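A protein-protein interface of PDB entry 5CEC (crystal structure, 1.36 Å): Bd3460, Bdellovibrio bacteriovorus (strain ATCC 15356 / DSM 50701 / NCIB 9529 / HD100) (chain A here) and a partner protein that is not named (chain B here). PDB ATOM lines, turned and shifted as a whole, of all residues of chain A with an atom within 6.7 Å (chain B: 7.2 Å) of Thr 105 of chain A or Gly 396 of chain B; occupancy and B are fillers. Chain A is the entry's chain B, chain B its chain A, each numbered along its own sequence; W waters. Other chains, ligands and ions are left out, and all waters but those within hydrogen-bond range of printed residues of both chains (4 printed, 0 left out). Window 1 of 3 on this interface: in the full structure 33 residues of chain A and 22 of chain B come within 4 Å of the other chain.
Thr 105 of chain A touches just one residue of chain B: Gly 396.
Of the printed residues of chain A, Gly 396 of chain B touches Thr 105 and Arg 137.
Printed residues of chain A within 4 Å of Arg 392 of chain B: Phe 102 (3.97 Å).
Of the printed residues of chain A, Val 397 of chain B touches Ala 127.
Of the printed residues of chain A, Ser 393 of chain B touches Glu 97, Phe 102 and Ala 127.
Printed residues of chain A within 4 Å of Trp 395 of chain B: Asn 106 (3.8 Å).
Val 39 of chain B touches none of the printed residues of chain A.
Ser 399 of chain B touches none of the printed residues of chain A.
The nearest residue of chain B that does not touch Thr 105 of chain A is Ser 399 of chain B (4.4 Å).
The nearest residue of chain A that does not touch Gly 396 of chain B is Asn 106 of chain A (4.3 Å).
Phe 102 of chain A touches Arg 392 of chain B.
Phe 102 of chain A touches Ser 393 of chain B (CZ to OG, 3.999 Å).
Thr 105 of chain A touches Gly 396 of chain B.
Trp 395 of chain B touches Asn 106 of chain A.
Ala 127 of chain A touches Ser 393 of chain B (CB to CB, 3.6 Å).
Ala 127 of chain A touches Val 397 of chain B.
Gly 396 of chain B touches Arg 137 of chain A (O to NH1, 3.7 Å).
CD of Arg 137 of chain A touches OE1 of Gln 400 of chain B, 3.2 Å away.
OE1 of Glu 97 of chain A lies within hydrogen-bond range of OG of Ser 393 of chain B, 2.7 Å away.
NZ of Lys 403 of chain B lies within salt-bridge range of OD2 of Asp 107 of chain A, 2.8 Å away.
Water W4 lies within hydrogen-bond range of the side-chain hydroxyl of Ser 399 of chain B (2.7 Å), the side-chain carboxylate of Asp 107 of chain A (2.8 Å) and the backbone carbonyl oxygen of Thr 105 of chain A (2.9 Å).
Water W1 lies within hydrogen-bond range of O of Thr 105 of chain A, O of Gly 396 of chain B and NH1 of Arg 137 of chain A.
Water W2 lies within hydrogen-bond range of the side-chain carboxylate of Glu 97 of chain A (2.8 Å), the backbone carbonyl oxygen of Ser 393 of chain B (3.0 Å) and the backbone NH of Val 397 of chain B (3.3 Å).
Water W3 lies within hydrogen-bond range of O of Arg 392 of chain B (2.8 Å), N of Gly 396 of chain B (2.9 Å), ND2 of Asn 106 of chain A (3.1 Å) and O of Ser 393 of chain B (3.5 Å).
Hydrophobic or aromatic side chains of chain B that line the printed part of chain A: Trp 395 and Val 397.
Along chain B the printed residues that touch a printed residue of chain A span positions 392 to 403.
Printed residues of chain A that touch a printed residue of chain B: Glu 97, Phe 102, Thr 105, Asn 106, Asp 107, Ala 127 and Arg 137.
The backbone carbonyl oxygen (O) of Tyr 388 of chain B sits at hydrogen-bond distance from the guanidinium group (NH1) of Arg 392 of chain B (3.1 Å).
The backbone carbonyl oxygen of Phe 102 of chain A is in hydrogen-bond range of the side-chain hydroxyl of Thr 105 of chain A, at 3.3 Å.
OE2 of Glu 97 of chain A sits at hydrogen-bond distance from N of Ala 127 of chain A, at 2.9 Å.
The backbone carbonyl oxygen of Ala 101 of chain A sits at hydrogen-bond distance from the side-chain hydroxyl of Thr 105 of chain A (2.8 Å).
ND2 of Asn 106 of chain A sits at hydrogen-bond distance from O of Phe 102 of chain A, at 3.0 Å.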
ATOM      1  N   GLU A  97     -10.023  30.123  14.210  1.00  0.00           N
ATOM      2  CA  GLU A  97      -8.698  29.619  13.911  1.00  0.00           C
ATOM      3  C   GLU A  97      -7.765  30.654  13.341  1.00  0.00           C
ATOM      4  O   GLU A  97      -8.100  31.385  12.415  1.00  0.00           O
ATOM      5  CB  GLU A  97      -8.798  28.430  12.967  1.00  0.00           C
ATOM      6  CG  GLU A  97      -9.393  27.203  13.647  1.00  0.00           C
ATOM      7  CD  GLU A  97      -9.390  25.951  12.788  1.00  0.00           C
ATOM      8  OE1 GLU A  97      -9.637  26.070  11.567  1.00  0.00           O
ATOM      9  OE2 GLU A  97      -9.156  24.858  13.356  1.00  0.00           O
ATOM     10  N   LEU A 100      -1.891  29.492  12.128  1.00  0.00           N
ATOM     11  CA  LEU A 100      -1.181  28.352  12.697  1.00  0.00           C
ATOM     12  C   LEU A 100      -2.143  27.196  12.950  1.00  0.00           C
ATOM     13  O   LEU A 100      -1.789  26.023  12.699  1.00  0.00           O
ATOM     14  CB  LEU A 100      -0.445  28.764  13.975  1.00  0.00           C
ATOM     15  CG  LEU A 100       0.286  27.628  14.696  1.00  0.00           C
ATOM     16  CD1 LEU A 100       1.286  26.882  13.801  1.00  0.00           C
ATOM     17  CD2 LEU A 100       1.007  28.179  15.922  1.00  0.00           C
ATOM     18  N   ALA A 101      -3.331  27.488  13.456  1.00  0.00           N
ATOM     19  CA  ALA A 101      -4.344  26.434  13.576  1.00  0.00           C
ATOM     20  C   ALA A 101      -4.718  25.830  12.250  1.00  0.00           C
ATOM     21  O   ALA A 101      -4.819  24.607  12.172  1.00  0.00           O
ATOM     22  CB  ALA A 101      -5.572  26.944  14.292  1.00  0.00           C
ATOM     23  N   PHE A 102      -4.879  26.622  11.218  1.00  0.00           N
ATOM     24  CA  PHE A 102      -5.126  26.077   9.872  1.00  0.00           C
ATOM     25  C   PHE A 102      -4.022  25.135   9.431  1.00  0.00           C
ATOM     26  O   PHE A 102      -4.300  24.071   8.885  1.00  0.00           O
ATOM     27  CB  PHE A 102      -5.313  27.180   8.839  1.00  0.00           C
ATOM     28  CG  PHE A 102      -6.696  27.721   8.779  1.00  0.00           C
ATOM     29  CD1 PHE A 102      -7.657  27.019   8.091  1.00  0.00           C
ATOM     30  CD2 PHE A 102      -7.072  28.916   9.411  1.00  0.00           C
ATOM     31  CE1 PHE A 102      -8.958  27.463   8.026  1.00  0.00           C
ATOM     32  CE2 PHE A 102      -8.386  29.376   9.303  1.00  0.00           C
ATOM     33  CZ  PHE A 102      -9.313  28.642   8.608  1.00  0.00           C
ATOM     34  N   ALA A 103      -2.773  25.512   9.684  1.00  0.00           N
ATOM     35  CA  ALA A 103      -1.645  24.693   9.252  1.00  0.00           C
ATOM     36  C   ALA A 103      -1.657  23.357   9.987  1.00  0.00           C
ATOM     37  O   ALA A 103      -1.582  22.299   9.364  1.00  0.00           O
ATOM     38  CB  ALA A 103      -0.336  25.416   9.497  1.00  0.00           C
ATOM     39  N   VAL A 104      -1.717  23.391  11.314  1.00  0.00           N
ATOM     40  CA  VAL A 104      -1.684  22.153  12.095  1.00  0.00           C
ATOM     41  C   VAL A 104      -2.840  21.255  11.718  1.00  0.00           C
ATOM     42  O   VAL A 104      -2.661  20.047  11.459  1.00  0.00           O
ATOM     43  CB  VAL A 104      -1.645  22.477  13.602  1.00  0.00           C
ATOM     44  CG1 VAL A 104      -1.956  21.255  14.439  1.00  0.00           C
ATOM     45  CG2 VAL A 104      -0.266  23.054  13.924  1.00  0.00           C
ATOM     46  N   THR A 105      -4.049  21.809  11.668  1.00  0.00           N
ATOM     47  CA  THR A 105      -5.225  20.976  11.439  1.00  0.00           C
ATOM     48  C   THR A 105      -5.305  20.417  10.023  1.00  0.00           C
ATOM     49  O   THR A 105      -5.981  19.412   9.816  1.00  0.00           O
ATOM     50  CB  THR A 105      -6.535  21.713  11.746  1.00  0.00           C
ATOM     51  OG1 THR A 105      -6.628  22.864  10.926  1.00  0.00           O
ATOM     52  CG2 THR A 105      -6.631  22.106  13.226  1.00  0.00           C
ATOM     53  N   ASN A 106      -4.621  21.034   9.068  1.00  0.00           N
ATOM     54  CA  ASN A 106      -4.528  20.505   7.715  1.00  0.00           C
ATOM     55  C   ASN A 106      -3.224  19.776   7.429  1.00  0.00           C
ATOM     56  O   ASN A 106      -2.920  19.514   6.274  1.00  0.00           O
ATOM     57  CB  ASN A 106      -4.798  21.621   6.701  1.00  0.00           C
ATOM     58  CG  ASN A 106      -6.275  21.996   6.625  1.00  0.00           C
ATOM     59  OD1 ASN A 106      -7.053  21.370   5.867  1.00  0.00           O
ATOM     60  ND2 ASN A 106      -6.684  23.004   7.399  1.00  0.00           N
ATOM     61  N   ASP A 107      -2.504  19.395   8.488  1.00  0.00           N
ATOM     62  CA  ASP A 107      -1.270  18.617   8.400  1.00  0.00           C
ATOM     63  C   ASP A 107      -0.180  19.301   7.588  1.00  0.00           C
ATOM     64  O   ASP A 107       0.727  18.646   7.082  1.00  0.00           O
ATOM     65  CB  ASP A 107      -1.528  17.194   7.875  1.00  0.00           C
ATOM     66  CG  ASP A 107      -2.329  16.327   8.821  1.00  0.00           C
ATOM     67  OD1 ASP A 107      -2.975  16.796   9.755  1.00  0.00           O
ATOM     68  OD2 ASP A 107      -2.336  15.107   8.661  1.00  0.00           O
ATOM     69  N   ALA A 108      -0.191  20.644   7.574  1.00  0.00           N
ATOM     70  CA  ALA A 108       0.868  21.435   6.963  1.00  0.00           C
ATOM     71  C   ALA A 108       1.895  21.775   8.036  1.00  0.00           C
ATOM     72  O   ALA A 108       2.025  22.904   8.480  1.00  0.00           O
ATOM     73  CB  ALA A 108       0.320  22.679   6.313  1.00  0.00           C
ATOM     74  N   TYR A 109       2.619  20.755   8.467  1.00  0.00           N
ATOM     75  CA  TYR A 109       3.515  20.892   9.599  1.00  0.00           C
ATOM     76  C   TYR A 109       4.810  21.621   9.275  1.00  0.00           C
ATOM     77  O   TYR A 109       5.373  22.253  10.160  1.00  0.00           O
ATOM     78  CB  TYR A 109       3.757  19.523  10.232  1.00  0.00           C
ATOM     79  CG  TYR A 109       2.578  19.117  11.094  1.00  0.00           C
ATOM     80  CD1 TYR A 109       2.366  19.722  12.327  1.00  0.00           C
ATOM     81  CD2 TYR A 109       1.633  18.168  10.670  1.00  0.00           C
ATOM     82  CE1 TYR A 109       1.292  19.394  13.133  1.00  0.00           C
ATOM     83  CE2 TYR A 109       0.544  17.838  11.465  1.00  0.00           C
ATOM     84  CZ  TYR A 109       0.376  18.441  12.698  1.00  0.00           C
ATOM     85  OH  TYR A 109      -0.662  18.122  13.533  1.00  0.00           O
ATOM     86  N   VAL A 126      -8.187  24.924  18.357  1.00  0.00           N
ATOM     87  CA  VAL A 126      -8.582  24.548  17.008  1.00  0.00           C
ATOM     88  C   VAL A 126     -10.103  24.330  16.984  1.00  0.00           C
ATOM     89  O   VAL A 126     -10.741  24.076  18.005  1.00  0.00           O
ATOM     90  CB  VAL A 126      -7.802  23.322  16.475  1.00  0.00           C
ATOM     91  CG1 VAL A 126      -6.296  23.592  16.541  1.00  0.00           C
ATOM     92  CG2 VAL A 126      -8.119  22.011  17.212  1.00  0.00           C
ATOM     93  N   ALA A 127     -10.643  24.391  15.793  1.00  0.00           N
ATOM     94  CA  ALA A 127     -12.080  24.312  15.609  1.00  0.00           C
ATOM     95  C   ALA A 127     -12.615  22.934  16.011  1.00  0.00           C
ATOM     96  O   ALA A 127     -11.875  21.937  16.026  1.00  0.00           O
ATOM     97  CB  ALA A 127     -12.446  24.595  14.158  1.00  0.00           C
ATOM     98  N   LEU A 134      -4.197  23.474  20.246  1.00  0.00           N
ATOM     99  CA  LEU A 134      -3.229  23.238  19.160  1.00  0.00           C
ATOM    100  C   LEU A 134      -2.260  22.105  19.526  1.00  0.00           C
ATOM    101  O   LEU A 134      -1.949  21.233  18.695  1.00  0.00           O
ATOM    102  CB  LEU A 134      -2.437  24.500  18.854  1.00  0.00           C
ATOM    103  CG  LEU A 134      -1.590  24.464  17.593  1.00  0.00           C
ATOM    104  CD1 LEU A 134      -2.491  24.660  16.371  1.00  0.00           C
ATOM    105  CD2 LEU A 134      -0.521  25.537  17.627  1.00  0.00           C
ATOM    106  N   ARG A 137      -3.749  18.586  19.075  1.00  0.00           N
ATOM    107  CA  ARG A 137      -3.869  18.192  17.698  1.00  0.00           C
ATOM    108  C   ARG A 137      -2.506  17.774  17.137  1.00  0.00           C
ATOM    109  O   ARG A 137      -2.373  16.749  16.445  1.00  0.00           O
ATOM    110  CB  ARG A 137      -4.535  19.301  16.869  1.00  0.00           C
ATOM    111  CG  ARG A 137      -4.821  18.910  15.425  1.00  0.00           C
ATOM    112  CD  ARG A 137      -5.704  17.681  15.254  1.00  0.00           C
ATOM    113  NE  ARG A 137      -6.902  17.773  16.098  1.00  0.00           N
ATOM    114  CZ  ARG A 137      -8.028  18.432  15.797  1.00  0.00           C
ATOM    115  NH1 ARG A 137      -8.192  18.971  14.607  1.00  0.00           N
ATOM    116  NH2 ARG A 137      -8.984  18.538  16.703  1.00  0.00           N
ATOM    117  N   VAL B  39     -19.864  19.491   9.969  1.00  0.00           N
ATOM    118  CA  VAL B  39     -19.236  18.219   9.691  1.00  0.00           C
ATOM    119  C   VAL B  39     -20.101  17.090  10.222  1.00  0.00           C
ATOM    120  O   VAL B  39     -20.509  17.129  11.379  1.00  0.00           O
ATOM    121  CB  VAL B  39     -17.836  18.175  10.315  1.00  0.00           C
ATOM    122  CG1 VAL B  39     -17.193  16.809  10.184  1.00  0.00           C
ATOM    123  CG2 VAL B  39     -16.997  19.291   9.687  1.00  0.00           C
ATOM    124  N   LYS B 365     -14.829  15.566   2.930  1.00  0.00           N
ATOM    125  CA  LYS B 365     -13.486  15.175   3.359  1.00  0.00           C
ATOM    126  C   LYS B 365     -13.515  13.656   3.369  1.00  0.00           C
ATOM    127  O   LYS B 365     -14.451  13.057   3.937  1.00  0.00           O
ATOM    128  CB  LYS B 365     -13.141  15.725   4.748  1.00  0.00           C
ATOM    129  CG  LYS B 365     -11.661  15.644   5.080  1.00  0.00           C
ATOM    130  CD  LYS B 365     -10.893  16.816   4.446  1.00  0.00           C
ATOM    131  CE  LYS B 365      -9.389  16.736   4.699  1.00  0.00           C
ATOM    132  NZ  LYS B 365      -8.832  15.643   3.854  1.00  0.00           N
ATOM    133  N   THR B 386     -18.772  18.043   4.615  1.00  0.00           N
ATOM    134  CA  THR B 386     -18.307  19.340   5.098  1.00  0.00           C
ATOM    135  C   THR B 386     -19.067  20.440   4.403  1.00  0.00           C
ATOM    136  O   THR B 386     -19.717  20.196   3.374  1.00  0.00           O
ATOM    137  CB  THR B 386     -16.792  19.540   4.848  1.00  0.00           C
ATOM    138  OG1 THR B 386     -16.464  19.355   3.472  1.00  0.00           O
ATOM    139  CG2 THR B 386     -15.959  18.518   5.622  1.00  0.00           C
ATOM    140  N   TYR B 388     -17.244  23.576   3.504  1.00  0.00           N
ATOM    141  CA  TYR B 388     -16.034  24.374   3.514  1.00  0.00           C
ATOM    142  C   TYR B 388     -16.289  25.821   3.050  1.00  0.00           C
ATOM    143  O   TYR B 388     -15.660  26.758   3.586  1.00  0.00           O
ATOM    144  CB  TYR B 388     -14.993  23.601   2.712  1.00  0.00           C
ATOM    145  CG  TYR B 388     -13.797  24.312   2.225  1.00  0.00           C
ATOM    146  CD1 TYR B 388     -13.838  25.067   1.042  1.00  0.00           C
ATOM    147  CD2 TYR B 388     -12.588  24.164   2.870  1.00  0.00           C
ATOM    148  CE1 TYR B 388     -12.693  25.668   0.539  1.00  0.00           C
ATOM    149  CE2 TYR B 388     -11.440  24.744   2.368  1.00  0.00           C
ATOM    150  CZ  TYR B 388     -11.497  25.503   1.210  1.00  0.00           C
ATOM    151  OH  TYR B 388     -10.337  26.107   0.757  1.00  0.00           O
ATOM    152  N   ARG B 392     -14.351  27.400   6.548  1.00  0.00           N
ATOM    153  CA  ARG B 392     -13.126  26.770   6.032  1.00  0.00           C
ATOM    154  C   ARG B 392     -12.513  25.847   7.062  1.00  0.00           C
ATOM    155  O   ARG B 392     -11.747  24.984   6.677  1.00  0.00           O
ATOM    156  CB  ARG B 392     -12.134  27.851   5.600  1.00  0.00           C
ATOM    157  CG  ARG B 392     -12.664  28.746   4.491  1.00  0.00           C
ATOM    158  CD  ARG B 392     -12.619  28.118   3.133  1.00  0.00           C
ATOM    159  NE  ARG B 392     -12.740  29.140   2.075  1.00  0.00           N
ATOM    160  CZ  ARG B 392     -13.866  29.740   1.663  1.00  0.00           C
ATOM    161  NH1 ARG B 392     -15.055  29.479   2.193  1.00  0.00           N
ATOM    162  NH2 ARG B 392     -13.803  30.610   0.684  1.00  0.00           N
ATOM    163  N   SER B 393     -12.840  26.015   8.356  1.00  0.00           N
ATOM    164  CA  SER B 393     -12.321  25.131   9.387  1.00  0.00           C
ATOM    165  C   SER B 393     -12.851  23.701   9.321  1.00  0.00           C
ATOM    166  O   SER B 393     -12.316  22.796   9.977  1.00  0.00           O
ATOM    167  CB  SER B 393     -12.651  25.720  10.768  1.00  0.00           C
ATOM    168  OG  SER B 393     -12.095  27.013  10.975  1.00  0.00           O
ATOM    169  N   ASP B 394     -13.890  23.474   8.526  1.00  0.00           N
ATOM    170  CA  ASP B 394     -14.501  22.132   8.447  1.00  0.00           C
ATOM    171  C   ASP B 394     -13.528  21.063   7.983  1.00  0.00           C
ATOM    172  O   ASP B 394     -13.660  19.945   8.450  1.00  0.00           O
ATOM    173  CB  ASP B 394     -15.721  22.119   7.517  1.00  0.00           C
ATOM    174  CG  ASP B 394     -16.985  22.652   8.132  1.00  0.00           C
ATOM    175  OD1 ASP B 394     -16.967  23.178   9.271  1.00  0.00           O
ATOM    176  OD2 ASP B 394     -18.040  22.498   7.447  1.00  0.00           O
ATOM    177  N   TRP B 395     -12.605  21.353   7.068  1.00  0.00           N
ATOM    178  CA  TRP B 395     -11.687  20.302   6.617  1.00  0.00           C
ATOM    179  C   TRP B 395     -10.850  19.765   7.776  1.00  0.00           C
ATOM    180  O   TRP B 395     -10.740  18.550   7.927  1.00  0.00           O
ATOM    181  CB  TRP B 395     -10.796  20.779   5.476  1.00  0.00           C
ATOM    182  CG  TRP B 395     -11.450  20.849   4.141  1.00  0.00           C
ATOM    183  CD1 TRP B 395     -12.747  20.482   3.804  1.00  0.00           C
ATOM    184  CD2 TRP B 395     -10.842  21.282   2.933  1.00  0.00           C
ATOM    185  NE1 TRP B 395     -12.945  20.677   2.479  1.00  0.00           N
ATOM    186  CE2 TRP B 395     -11.807  21.175   1.914  1.00  0.00           C
ATOM    187  CE3 TRP B 395      -9.564  21.737   2.596  1.00  0.00           C
ATOM    188  CZ2 TRP B 395     -11.544  21.521   0.616  1.00  0.00           C
ATOM    189  CZ3 TRP B 395      -9.306  22.058   1.291  1.00  0.00           C
ATOM    190  CH2 TRP B 395     -10.303  21.965   0.318  1.00  0.00           C
ATOM    191  N   GLY B 396     -10.297  20.648   8.586  1.00  0.00           N
ATOM    192  CA  GLY B 396      -9.501  20.184   9.698  1.00  0.00           C
ATOM    193  C   GLY B 396     -10.302  19.436  10.742  1.00  0.00           C
ATOM    194  O   GLY B 396      -9.858  18.450  11.299  1.00  0.00           O
ATOM    195  N   VAL B 397     -11.535  19.870  10.982  1.00  0.00           N
ATOM    196  CA  VAL B 397     -12.405  19.175  11.909  1.00  0.00           C
ATOM    197  C   VAL B 397     -12.704  17.768  11.381  1.00  0.00           C
ATOM    198  O   VAL B 397     -12.564  16.756  12.084  1.00  0.00           O
ATOM    199  CB  VAL B 397     -13.735  19.948  12.127  1.00  0.00           C
ATOM    200  CG1 VAL B 397     -14.735  19.131  12.917  1.00  0.00           C
ATOM    201  CG2 VAL B 397     -13.445  21.269  12.858  1.00  0.00           C
ATOM    202  N   ALA B 398     -13.126  17.691  10.127  1.00  0.00           N
ATOM    203  CA  ALA B 398     -13.433  16.373   9.523  1.00  0.00           C
ATOM    204  C   ALA B 398     -12.215  15.474   9.490  1.00  0.00           C
ATOM    205  O   ALA B 398     -12.343  14.267   9.693  1.00  0.00           O
ATOM    206  CB  ALA B 398     -13.993  16.576   8.127  1.00  0.00           C
ATOM    207  N   SER B 399     -11.054  16.048   9.206  1.00  0.00           N
ATOM    208  CA  SER B 399      -9.863  15.228   9.084  1.00  0.00           C
ATOM    209  C   SER B 399      -9.602  14.451  10.381  1.00  0.00           C
ATOM    210  O   SER B 399      -9.317  13.249  10.332  1.00  0.00           O
ATOM    211  CB  SER B 399      -8.645  16.091   8.788  1.00  0.00           C
ATOM    212  OG  SER B 399      -7.517  15.256   8.602  1.00  0.00           O
ATOM    213  N   GLN B 400      -9.638  15.123  11.521  1.00  0.00           N
ATOM    214  CA  GLN B 400      -9.366  14.421  12.763  1.00  0.00           C
ATOM    215  C   GLN B 400     -10.491  13.446  13.107  1.00  0.00           C
ATOM    216  O   GLN B 400     -10.223  12.363  13.645  1.00  0.00           O
ATOM    217  CB  GLN B 400      -9.049  15.351  13.921  1.00  0.00           C
ATOM    218  CG  GLN B 400      -8.466  14.614  15.150  1.00  0.00           C
ATOM    219  CD  GLN B 400      -7.143  13.960  14.866  1.00  0.00           C
ATOM    220  OE1 GLN B 400      -6.195  14.599  14.437  1.00  0.00           O
ATOM    221  NE2 GLN B 400      -7.039  12.666  15.168  1.00  0.00           N
ATOM    222  N   GLN B 401     -11.731  13.774  12.778  1.00  0.00           N
ATOM    223  CA  GLN B 401     -12.810  12.803  12.971  1.00  0.00           C
ATOM    224  C   GLN B 401     -12.584  11.537  12.155  1.00  0.00           C
ATOM    225  O   GLN B 401     -12.806  10.435  12.668  1.00  0.00           O
ATOM    226  CB  GLN B 401     -14.175  13.408  12.672  1.00  0.00           C
ATOM    227  CG  GLN B 401     -14.656  14.394  13.715  1.00  0.00           C
ATOM    228  CD  GLN B 401     -16.051  14.907  13.439  1.00  0.00           C
ATOM    229  OE1 GLN B 401     -16.827  14.289  12.713  1.00  0.00           O
ATOM    230  NE2 GLN B 401     -16.401  16.014  14.071  1.00  0.00           N
ATOM    231  N   ILE B 402     -12.139  11.678  10.905  1.00  0.00           N
ATOM    232  CA  ILE B 402     -11.817  10.529  10.084  1.00  0.00           C
ATOM    233  C   ILE B 402     -10.698   9.717  10.721  1.00  0.00           C
ATOM    234  O   ILE B 402     -10.793   8.509  10.839  1.00  0.00           O
ATOM    235  CB  ILE B 402     -11.431  10.944   8.652  1.00  0.00           C
ATOM    236  CG1 ILE B 402     -12.636  11.551   7.908  1.00  0.00           C
ATOM    237  CG2 ILE B 402     -10.865   9.747   7.895  1.00  0.00           C
ATOM    238  CD1 ILE B 402     -12.277  12.205   6.611  1.00  0.00           C
ATOM    239  N   LYS B 403      -9.619  10.381  11.129  1.00  0.00           N
ATOM    240  CA  LYS B 403      -8.495   9.677  11.732  1.00  0.00           C
ATOM    241  C   LYS B 403      -8.927   8.886  12.950  1.00  0.00           C
ATOM    242  O   LYS B 403      -8.519   7.734  13.135  1.00  0.00           O
ATOM    243  CB  LYS B 403      -7.419  10.688  12.143  1.00  0.00           C
ATOM    244  CG  LYS B 403      -6.736  11.344  10.978  1.00  0.00           C
ATOM    245  CD  LYS B 403      -5.691  12.360  11.425  1.00  0.00           C
ATOM    246  CE  LYS B 403      -4.989  13.019  10.249  1.00  0.00           C
ATOM    247  NZ  LYS B 403      -4.002  14.022  10.689  1.00  0.00           N
HETATM  248  O   HOH W   1      -7.206  18.126  11.896  1.00  0.00           O
HETATM  249  O   HOH W   2     -10.037  22.687  11.892  1.00  0.00           O
HETATM  250  O   HOH W   3      -9.713  23.362   7.736  1.00  0.00           O
HETATM  251  O   HOH W   4      -5.478  16.946   8.459  1.00  0.00           O
